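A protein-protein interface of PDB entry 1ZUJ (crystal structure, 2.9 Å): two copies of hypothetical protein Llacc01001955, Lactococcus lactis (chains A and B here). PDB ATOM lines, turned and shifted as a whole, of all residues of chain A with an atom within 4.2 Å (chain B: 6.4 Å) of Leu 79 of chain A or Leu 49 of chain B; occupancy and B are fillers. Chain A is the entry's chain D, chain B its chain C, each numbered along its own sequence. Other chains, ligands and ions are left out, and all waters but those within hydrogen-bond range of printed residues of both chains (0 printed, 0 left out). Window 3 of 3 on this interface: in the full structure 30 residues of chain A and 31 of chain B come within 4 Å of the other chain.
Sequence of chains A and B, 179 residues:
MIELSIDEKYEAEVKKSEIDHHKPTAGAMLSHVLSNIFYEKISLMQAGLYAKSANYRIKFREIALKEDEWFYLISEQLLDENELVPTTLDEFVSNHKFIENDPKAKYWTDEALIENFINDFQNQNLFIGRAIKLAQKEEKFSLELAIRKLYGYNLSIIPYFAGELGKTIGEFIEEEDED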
ATOM      1  N   SER A  75      18.499  -9.065   1.465  1.00  0.00           N
ATOM      2  CA  SER A  75      19.010 -10.200   0.684  1.00  0.00           C
ATOM      3  C   SER A  75      20.153 -10.927   1.385  1.00  0.00           C
ATOM      4  O   SER A  75      20.126 -12.146   1.467  1.00  0.00           O
ATOM      5  CB  SER A  75      19.484  -9.746  -0.700  1.00  0.00           C
ATOM      6  OG  SER A  75      18.423  -9.194  -1.458  1.00  0.00           O
ATOM      7  N   GLU A  76      21.153 -10.186   1.869  1.00  0.00           N
ATOM      8  CA  GLU A  76      22.270 -10.772   2.596  1.00  0.00           C
ATOM      9  C   GLU A  76      21.782 -11.401   3.857  1.00  0.00           C
ATOM     10  O   GLU A  76      22.343 -12.356   4.331  1.00  0.00           O
ATOM     11  CB  GLU A  76      23.249  -9.732   3.073  1.00  0.00           C
ATOM     12  CG  GLU A  76      23.562  -8.606   2.150  1.00  0.00           C
ATOM     13  CD  GLU A  76      25.000  -8.213   2.270  1.00  0.00           C
ATOM     14  OE1 GLU A  76      25.257  -7.017   2.564  1.00  0.00           O
ATOM     15  OE2 GLU A  76      25.861  -9.113   2.079  1.00  0.00           O
ATOM     16  N   GLN A  77      20.784 -10.789   4.464  1.00  0.00           N
ATOM     17  CA  GLN A  77      20.170 -11.345   5.655  1.00  0.00           C
ATOM     18  C   GLN A  77      19.657 -12.761   5.381  1.00  0.00           C
ATOM     19  O   GLN A  77      19.857 -13.675   6.165  1.00  0.00           O
ATOM     20  CB  GLN A  77      19.005 -10.462   6.074  1.00  0.00           C
ATOM     21  CG  GLN A  77      18.966 -10.161   7.561  1.00  0.00           C
ATOM     22  CD  GLN A  77      20.168  -9.394   8.033  1.00  0.00           C
ATOM     23  OE1 GLN A  77      20.456  -9.382   9.228  1.00  0.00           O
ATOM     24  NE2 GLN A  77      20.871  -8.751   7.107  1.00  0.00           N
ATOM     25  N   LEU A  78      18.982 -12.896   4.246  1.00  0.00           N
ATOM     26  CA  LEU A  78      18.357 -14.122   3.822  1.00  0.00           C
ATOM     27  C   LEU A  78      19.462 -15.069   3.402  1.00  0.00           C
ATOM     28  O   LEU A  78      19.392 -16.265   3.635  1.00  0.00           O
ATOM     29  CB  LEU A  78      17.429 -13.832   2.635  1.00  0.00           C
ATOM     30  CG  LEU A  78      15.909 -14.078   2.662  1.00  0.00           C
ATOM     31  CD1 LEU A  78      15.310 -14.055   4.058  1.00  0.00           C
ATOM     32  CD2 LEU A  78      15.168 -13.054   1.755  1.00  0.00           C
ATOM     33  N   LEU A  79      20.509 -14.556   2.786  1.00  0.00           N
ATOM     34  CA  LEU A  79      21.591 -15.441   2.369  1.00  0.00           C
ATOM     35  C   LEU A  79      22.216 -16.106   3.594  1.00  0.00           C
ATOM     36  O   LEU A  79      22.520 -17.286   3.577  1.00  0.00           O
ATOM     37  CB  LEU A  79      22.661 -14.672   1.565  1.00  0.00           C
ATOM     38  CG  LEU A  79      22.319 -14.193   0.145  1.00  0.00           C
ATOM     39  CD1 LEU A  79      23.489 -14.327  -0.783  1.00  0.00           C
ATOM     40  CD2 LEU A  79      21.195 -14.986  -0.424  1.00  0.00           C
ATOM     41  N   ASP A  80      22.366 -15.333   4.667  1.00  0.00           N
ATOM     42  CA  ASP A  80      23.020 -15.796   5.872  1.00  0.00           C
ATOM     43  C   ASP A  80      22.230 -16.971   6.443  1.00  0.00           C
ATOM     44  O   ASP A  80      22.812 -17.898   7.017  1.00  0.00           O
ATOM     45  CB  ASP A  80      23.177 -14.655   6.887  1.00  0.00           C
ATOM     46  CG  ASP A  80      24.198 -13.584   6.451  1.00  0.00           C
ATOM     47  OD1 ASP A  80      24.791 -13.642   5.342  1.00  0.00           O
ATOM     48  OD2 ASP A  80      24.475 -12.613   7.157  1.00  0.00           O
ATOM     49  N   GLU A  81      20.917 -16.961   6.250  1.00  0.00           N
ATOM     50  CA  GLU A  81      20.073 -18.058   6.703  1.00  0.00           C
ATOM     51  C   GLU A  81      19.881 -19.123   5.610  1.00  0.00           C
ATOM     52  O   GLU A  81      18.964 -19.928   5.687  1.00  0.00           O
ATOM     53  CB  GLU A  81      18.715 -17.543   7.222  1.00  0.00           C
ATOM     54  CG  GLU A  81      18.815 -16.442   8.270  1.00  0.00           C
ATOM     55  CD  GLU A  81      18.780 -16.933   9.719  1.00  0.00           C
ATOM     56  OE1 GLU A  81      18.971 -18.148   9.974  1.00  0.00           O
ATOM     57  OE2 GLU A  81      18.556 -16.077  10.623  1.00  0.00           O
ATOM     58  N   ASN A  82      20.784 -19.149   4.634  1.00  0.00           N
ATOM     59  CA  ASN A  82      20.743 -20.103   3.522  1.00  0.00           C
ATOM     60  C   ASN A  82      19.387 -20.093   2.818  1.00  0.00           C
ATOM     61  O   ASN A  82      18.712 -21.111   2.714  1.00  0.00           O
ATOM     62  CB  ASN A  82      21.113 -21.517   3.991  1.00  0.00           C
ATOM     63  CG  ASN A  82      21.502 -22.448   2.823  1.00  0.00           C
ATOM     64  OD1 ASN A  82      22.608 -22.973   2.759  1.00  0.00           O
ATOM     65  ND2 ASN A  82      20.576 -22.641   1.891  1.00  0.00           N
ATOM     66  N   GLU A  83      18.987 -18.925   2.337  1.00  0.00           N
ATOM     67  CA  GLU A  83      17.725 -18.797   1.662  1.00  0.00           C
ATOM     68  C   GLU A  83      17.874 -18.221   0.262  1.00  0.00           C
ATOM     69  O   GLU A  83      18.839 -17.535  -0.046  1.00  0.00           O
ATOM     70  CB  GLU A  83      16.789 -17.984   2.533  1.00  0.00           C
ATOM     71  CG  GLU A  83      16.313 -18.801   3.727  1.00  0.00           C
ATOM     72  CD  GLU A  83      14.917 -19.381   3.545  1.00  0.00           C
ATOM     73  OE1 GLU A  83      14.326 -19.809   4.557  1.00  0.00           O
ATOM     74  OE2 GLU A  83      14.398 -19.381   2.399  1.00  0.00           O
ATOM     75  N   VAL A  85      17.190 -16.014  -2.969  1.00  0.00           N
ATOM     76  CA  VAL A  85      16.917 -14.609  -3.168  1.00  0.00           C
ATOM     77  C   VAL A  85      16.637 -14.415  -4.646  1.00  0.00           C
ATOM     78  O   VAL A  85      17.416 -14.900  -5.459  1.00  0.00           O
ATOM     79  CB  VAL A  85      18.136 -13.762  -2.719  1.00  0.00           C
ATOM     80  CG1 VAL A  85      18.045 -12.339  -3.234  1.00  0.00           C
ATOM     81  CG2 VAL A  85      18.241 -13.747  -1.200  1.00  0.00           C
ATOM     82  N   LEU B  44      25.123  -7.518 -12.120  1.00  0.00           N
ATOM     83  CA  LEU B  44      26.149  -7.108 -11.208  1.00  0.00           C
ATOM     84  C   LEU B  44      25.699  -7.317  -9.772  1.00  0.00           C
ATOM     85  O   LEU B  44      26.473  -7.772  -8.930  1.00  0.00           O
ATOM     86  CB  LEU B  44      26.478  -5.650 -11.445  1.00  0.00           C
ATOM     87  CG  LEU B  44      27.307  -5.389 -12.698  1.00  0.00           C
ATOM     88  CD1 LEU B  44      27.217  -3.937 -13.035  1.00  0.00           C
ATOM     89  CD2 LEU B  44      28.745  -5.777 -12.454  1.00  0.00           C
ATOM     90  N   MET B  45      24.441  -6.983  -9.501  1.00  0.00           N
ATOM     91  CA  MET B  45      23.850  -7.127  -8.168  1.00  0.00           C
ATOM     92  C   MET B  45      23.898  -8.599  -7.815  1.00  0.00           C
ATOM     93  O   MET B  45      24.298  -8.983  -6.720  1.00  0.00           O
ATOM     94  CB  MET B  45      22.386  -6.648  -8.167  1.00  0.00           C
ATOM     95  CG  MET B  45      21.977  -5.811  -6.951  1.00  0.00           C
ATOM     96  SD  MET B  45      21.294  -4.103  -7.354  1.00  0.00           S
ATOM     97  CE  MET B  45      19.830  -4.051  -6.236  1.00  0.00           C
ATOM     98  N   GLN B  46      23.497  -9.417  -8.776  1.00  0.00           N
ATOM     99  CA  GLN B  46      23.346 -10.819  -8.556  1.00  0.00           C
ATOM    100  C   GLN B  46      24.705 -11.360  -8.204  1.00  0.00           C
ATOM    101  O   GLN B  46      24.825 -12.278  -7.404  1.00  0.00           O
ATOM    102  CB  GLN B  46      22.811 -11.497  -9.815  1.00  0.00           C
ATOM    103  CG  GLN B  46      23.142 -12.988  -9.867  1.00  0.00           C
ATOM    104  CD  GLN B  46      22.567 -13.674 -11.048  1.00  0.00           C
ATOM    105  OE1 GLN B  46      21.664 -14.498 -10.909  1.00  0.00           O
ATOM    106  NE2 GLN B  46      23.098 -13.366 -12.217  1.00  0.00           N
ATOM    107  N   ALA B  47      25.726 -10.804  -8.836  1.00  0.00           N
ATOM    108  CA  ALA B  47      27.089 -11.230  -8.606  1.00  0.00           C
ATOM    109  C   ALA B  47      27.548 -10.652  -7.278  1.00  0.00           C
ATOM    110  O   ALA B  47      28.271 -11.291  -6.540  1.00  0.00           O
ATOM    111  CB  ALA B  47      27.982 -10.759  -9.742  1.00  0.00           C
ATOM    112  N   GLY B  48      27.096  -9.435  -6.978  1.00  0.00           N
ATOM    113  CA  GLY B  48      27.348  -8.779  -5.707  1.00  0.00           C
ATOM    114  C   GLY B  48      26.806  -9.518  -4.496  1.00  0.00           C
ATOM    115  O   GLY B  48      27.207  -9.235  -3.365  1.00  0.00           O
ATOM    116  N   LEU B  49      25.906 -10.463  -4.716  1.00  0.00           N
ATOM    117  CA  LEU B  49      25.404 -11.277  -3.630  1.00  0.00           C
ATOM    118  C   LEU B  49      25.991 -12.670  -3.605  1.00  0.00           C
ATOM    119  O   LEU B  49      26.306 -13.168  -2.519  1.00  0.00           O
ATOM    120  CB  LEU B  49      23.880 -11.341  -3.678  1.00  0.00           C
ATOM    121  CG  LEU B  49      23.282 -10.052  -3.081  1.00  0.00           C
ATOM    122  CD1 LEU B  49      22.204  -9.505  -3.942  1.00  0.00           C
ATOM    123  CD2 LEU B  49      22.747 -10.305  -1.714  1.00  0.00           C
ATOM    124  N   TYR B  50      26.176 -13.284  -4.777  1.00  0.00           N
ATOM    125  CA  TYR B  50      26.462 -14.715  -4.858  1.00  0.00           C
ATOM    126  C   TYR B  50      27.896 -15.090  -5.186  1.00  0.00           C
ATOM    127  O   TYR B  50      28.329 -16.215  -4.877  1.00  0.00           O
ATOM    128  CB  TYR B  50      25.548 -15.350  -5.873  1.00  0.00           C
ATOM    129  CG  TYR B  50      24.239 -15.720  -5.308  1.00  0.00           C
ATOM    130  CD1 TYR B  50      24.075 -16.920  -4.650  1.00  0.00           C
ATOM    131  CD2 TYR B  50      23.151 -14.889  -5.436  1.00  0.00           C
ATOM    132  CE1 TYR B  50      22.854 -17.291  -4.107  1.00  0.00           C
ATOM    133  CE2 TYR B  50      21.921 -15.245  -4.913  1.00  0.00           C
ATOM    134  CZ  TYR B  50      21.779 -16.456  -4.236  1.00  0.00           C
ATOM    135  OH  TYR B  50      20.551 -16.843  -3.708  1.00  0.00           O
ATOM    136  N   ALA B  51      28.629 -14.185  -5.829  1.00  0.00           N
ATOM    137  CA  ALA B  51      30.058 -14.419  -6.068  1.00  0.00           C
ATOM    138  C   ALA B  51      30.683 -14.971  -4.800  1.00  0.00           C
ATOM    139  O   ALA B  51      30.088 -14.894  -3.722  1.00  0.00           O
ATOM    140  CB  ALA B  51      30.795 -13.145  -6.517  1.00  0.00           C
ATOM    141  N   ARG B  57      32.769  -9.601  -4.656  1.00  0.00           N
ATOM    142  CA  ARG B  57      31.433  -9.142  -4.240  1.00  0.00           C
ATOM    143  C   ARG B  57      31.343  -7.618  -4.043  1.00  0.00           C
ATOM    144  O   ARG B  57      30.351  -7.001  -4.391  1.00  0.00           O
ATOM    145  CB  ARG B  57      31.011  -9.825  -2.943  1.00  0.00           C
ATOM    146  CG  ARG B  57      30.194 -11.103  -3.118  1.00  0.00           C
ATOM    147  CD  ARG B  57      29.535 -11.599  -1.815  1.00  0.00           C
ATOM    148  NE  ARG B  57      30.232 -12.745  -1.193  1.00  0.00           N
ATOM    149  CZ  ARG B  57      31.058 -12.678  -0.149  1.00  0.00           C
ATOM    150  NH1 ARG B  57      31.610 -13.775   0.338  1.00  0.00           N
ATOM    151  NH2 ARG B  57      31.351 -11.527   0.418  1.00  0.00           N
ATOM    152  N   PHE B  60      31.719  -5.841  -7.566  1.00  0.00           N
ATOM    153  CA  PHE B  60      30.466  -6.034  -8.275  1.00  0.00           C
ATOM    154  C   PHE B  60      29.420  -5.018  -7.827  1.00  0.00           C
ATOM    155  O   PHE B  60      28.584  -4.613  -8.628  1.00  0.00           O
ATOM    156  CB  PHE B  60      29.971  -7.474  -8.117  1.00  0.00           C
ATOM    157  CG  PHE B  60      30.791  -8.495  -8.881  1.00  0.00           C
ATOM    158  CD1 PHE B  60      31.367  -8.197 -10.118  1.00  0.00           C
ATOM    159  CD2 PHE B  60      30.973  -9.768  -8.381  1.00  0.00           C
ATOM    160  CE1 PHE B  60      32.109  -9.157 -10.822  1.00  0.00           C
ATOM    161  CE2 PHE B  60      31.717 -10.717  -9.090  1.00  0.00           C
ATOM    162  CZ  PHE B  60      32.280 -10.403 -10.311  1.00  0.00           C
ATOM    163  N   ARG B  61      29.488  -4.606  -6.556  1.00  0.00           N
ATOM    164  CA  ARG B  61      28.624  -3.560  -5.999  1.00  0.00           C
ATOM    165  C   ARG B  61      29.105  -2.131  -6.279  1.00  0.00           C
ATOM    166  O   ARG B  61      28.309  -1.274  -6.672  1.00  0.00           O
ATOM    167  CB  ARG B  61      28.471  -3.742  -4.500  1.00  0.00           C
ATOM    168  CG  ARG B  61      27.172  -4.351  -4.157  1.00  0.00           C
ATOM    169  CD  ARG B  61      26.931  -4.563  -2.689  1.00  0.00           C
ATOM    170  NE  ARG B  61      27.330  -5.906  -2.264  1.00  0.00           N
ATOM    171  CZ  ARG B  61      26.805  -6.565  -1.231  1.00  0.00           C
ATOM    172  NH1 ARG B  61      25.834  -6.027  -0.473  1.00  0.00           N
ATOM    173  NH2 ARG B  61      27.259  -7.784  -0.959  1.00  0.00           N
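NH1 of Arg 61 of chain B is in salt-bridge range of OE1 of Glu 76 of chain A (3.2 Å).
The guanidinium group (NH2) of Arg 61 of chain B sits at hydrogen-bond distance from the backbone carbonyl oxygen (O) of Gly 48 of chain B, at 2.8 Å.
CB of Ser 75 of chain A touches CD2 of Leu 49 of chain B, 3.5 Å away.
N of Glu 76 of chain A touches CD2 of Leu 49 of chain B, 3.9 Å away.
Leu 79 of chain A touches Leu 49 of chain B.
OH of Tyr 50 of chain B touches CD2 of Leu 79 of chain A, at 3.8 Å.
Val 85 of chain A touches Tyr 50 of chain B.
Leu 79 of chain A touches just these residues of chain B: Leu 49 and Tyr 50.
Of the printed residues of chain A, Arg 61 of chain B touches Glu 76.
Printed residues of chain A within 4 Å of Tyr 50 of chain B: Leu 79 and Val 85.
Printed residues of chain B within 4 Å of Ser 75 of chain A: Leu 49.
Of the printed residues of chain B, Glu 76 of chain A touches Leu 49 and Arg 61.
Of the printed residues of chain B, Val 85 of chain A touches Tyr 50 (3.5 Å).
Gln 46 of chain B touches none of the printed residues of chain A.
Ala 47 of chain B touches none of the printed residues of chain A.
The nearest printed residue of chain A that does not touch Leu 49 of chain B is Val 85 of chain A (5.1 Å).
Of the 11 printed residues of chain B, 3 touch a printed residue of chain A.
Hydrophobic or aromatic side chains of chain A that line the printed part of chain B: Leu 79.
Among the printed residues, Asp or Glu carboxylates within 4 Å of a Lys or Arg side-chain nitrogen of the other chain: Glu 76 of chain A with Arg 61 of chain B.
No position is printed for both chains.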
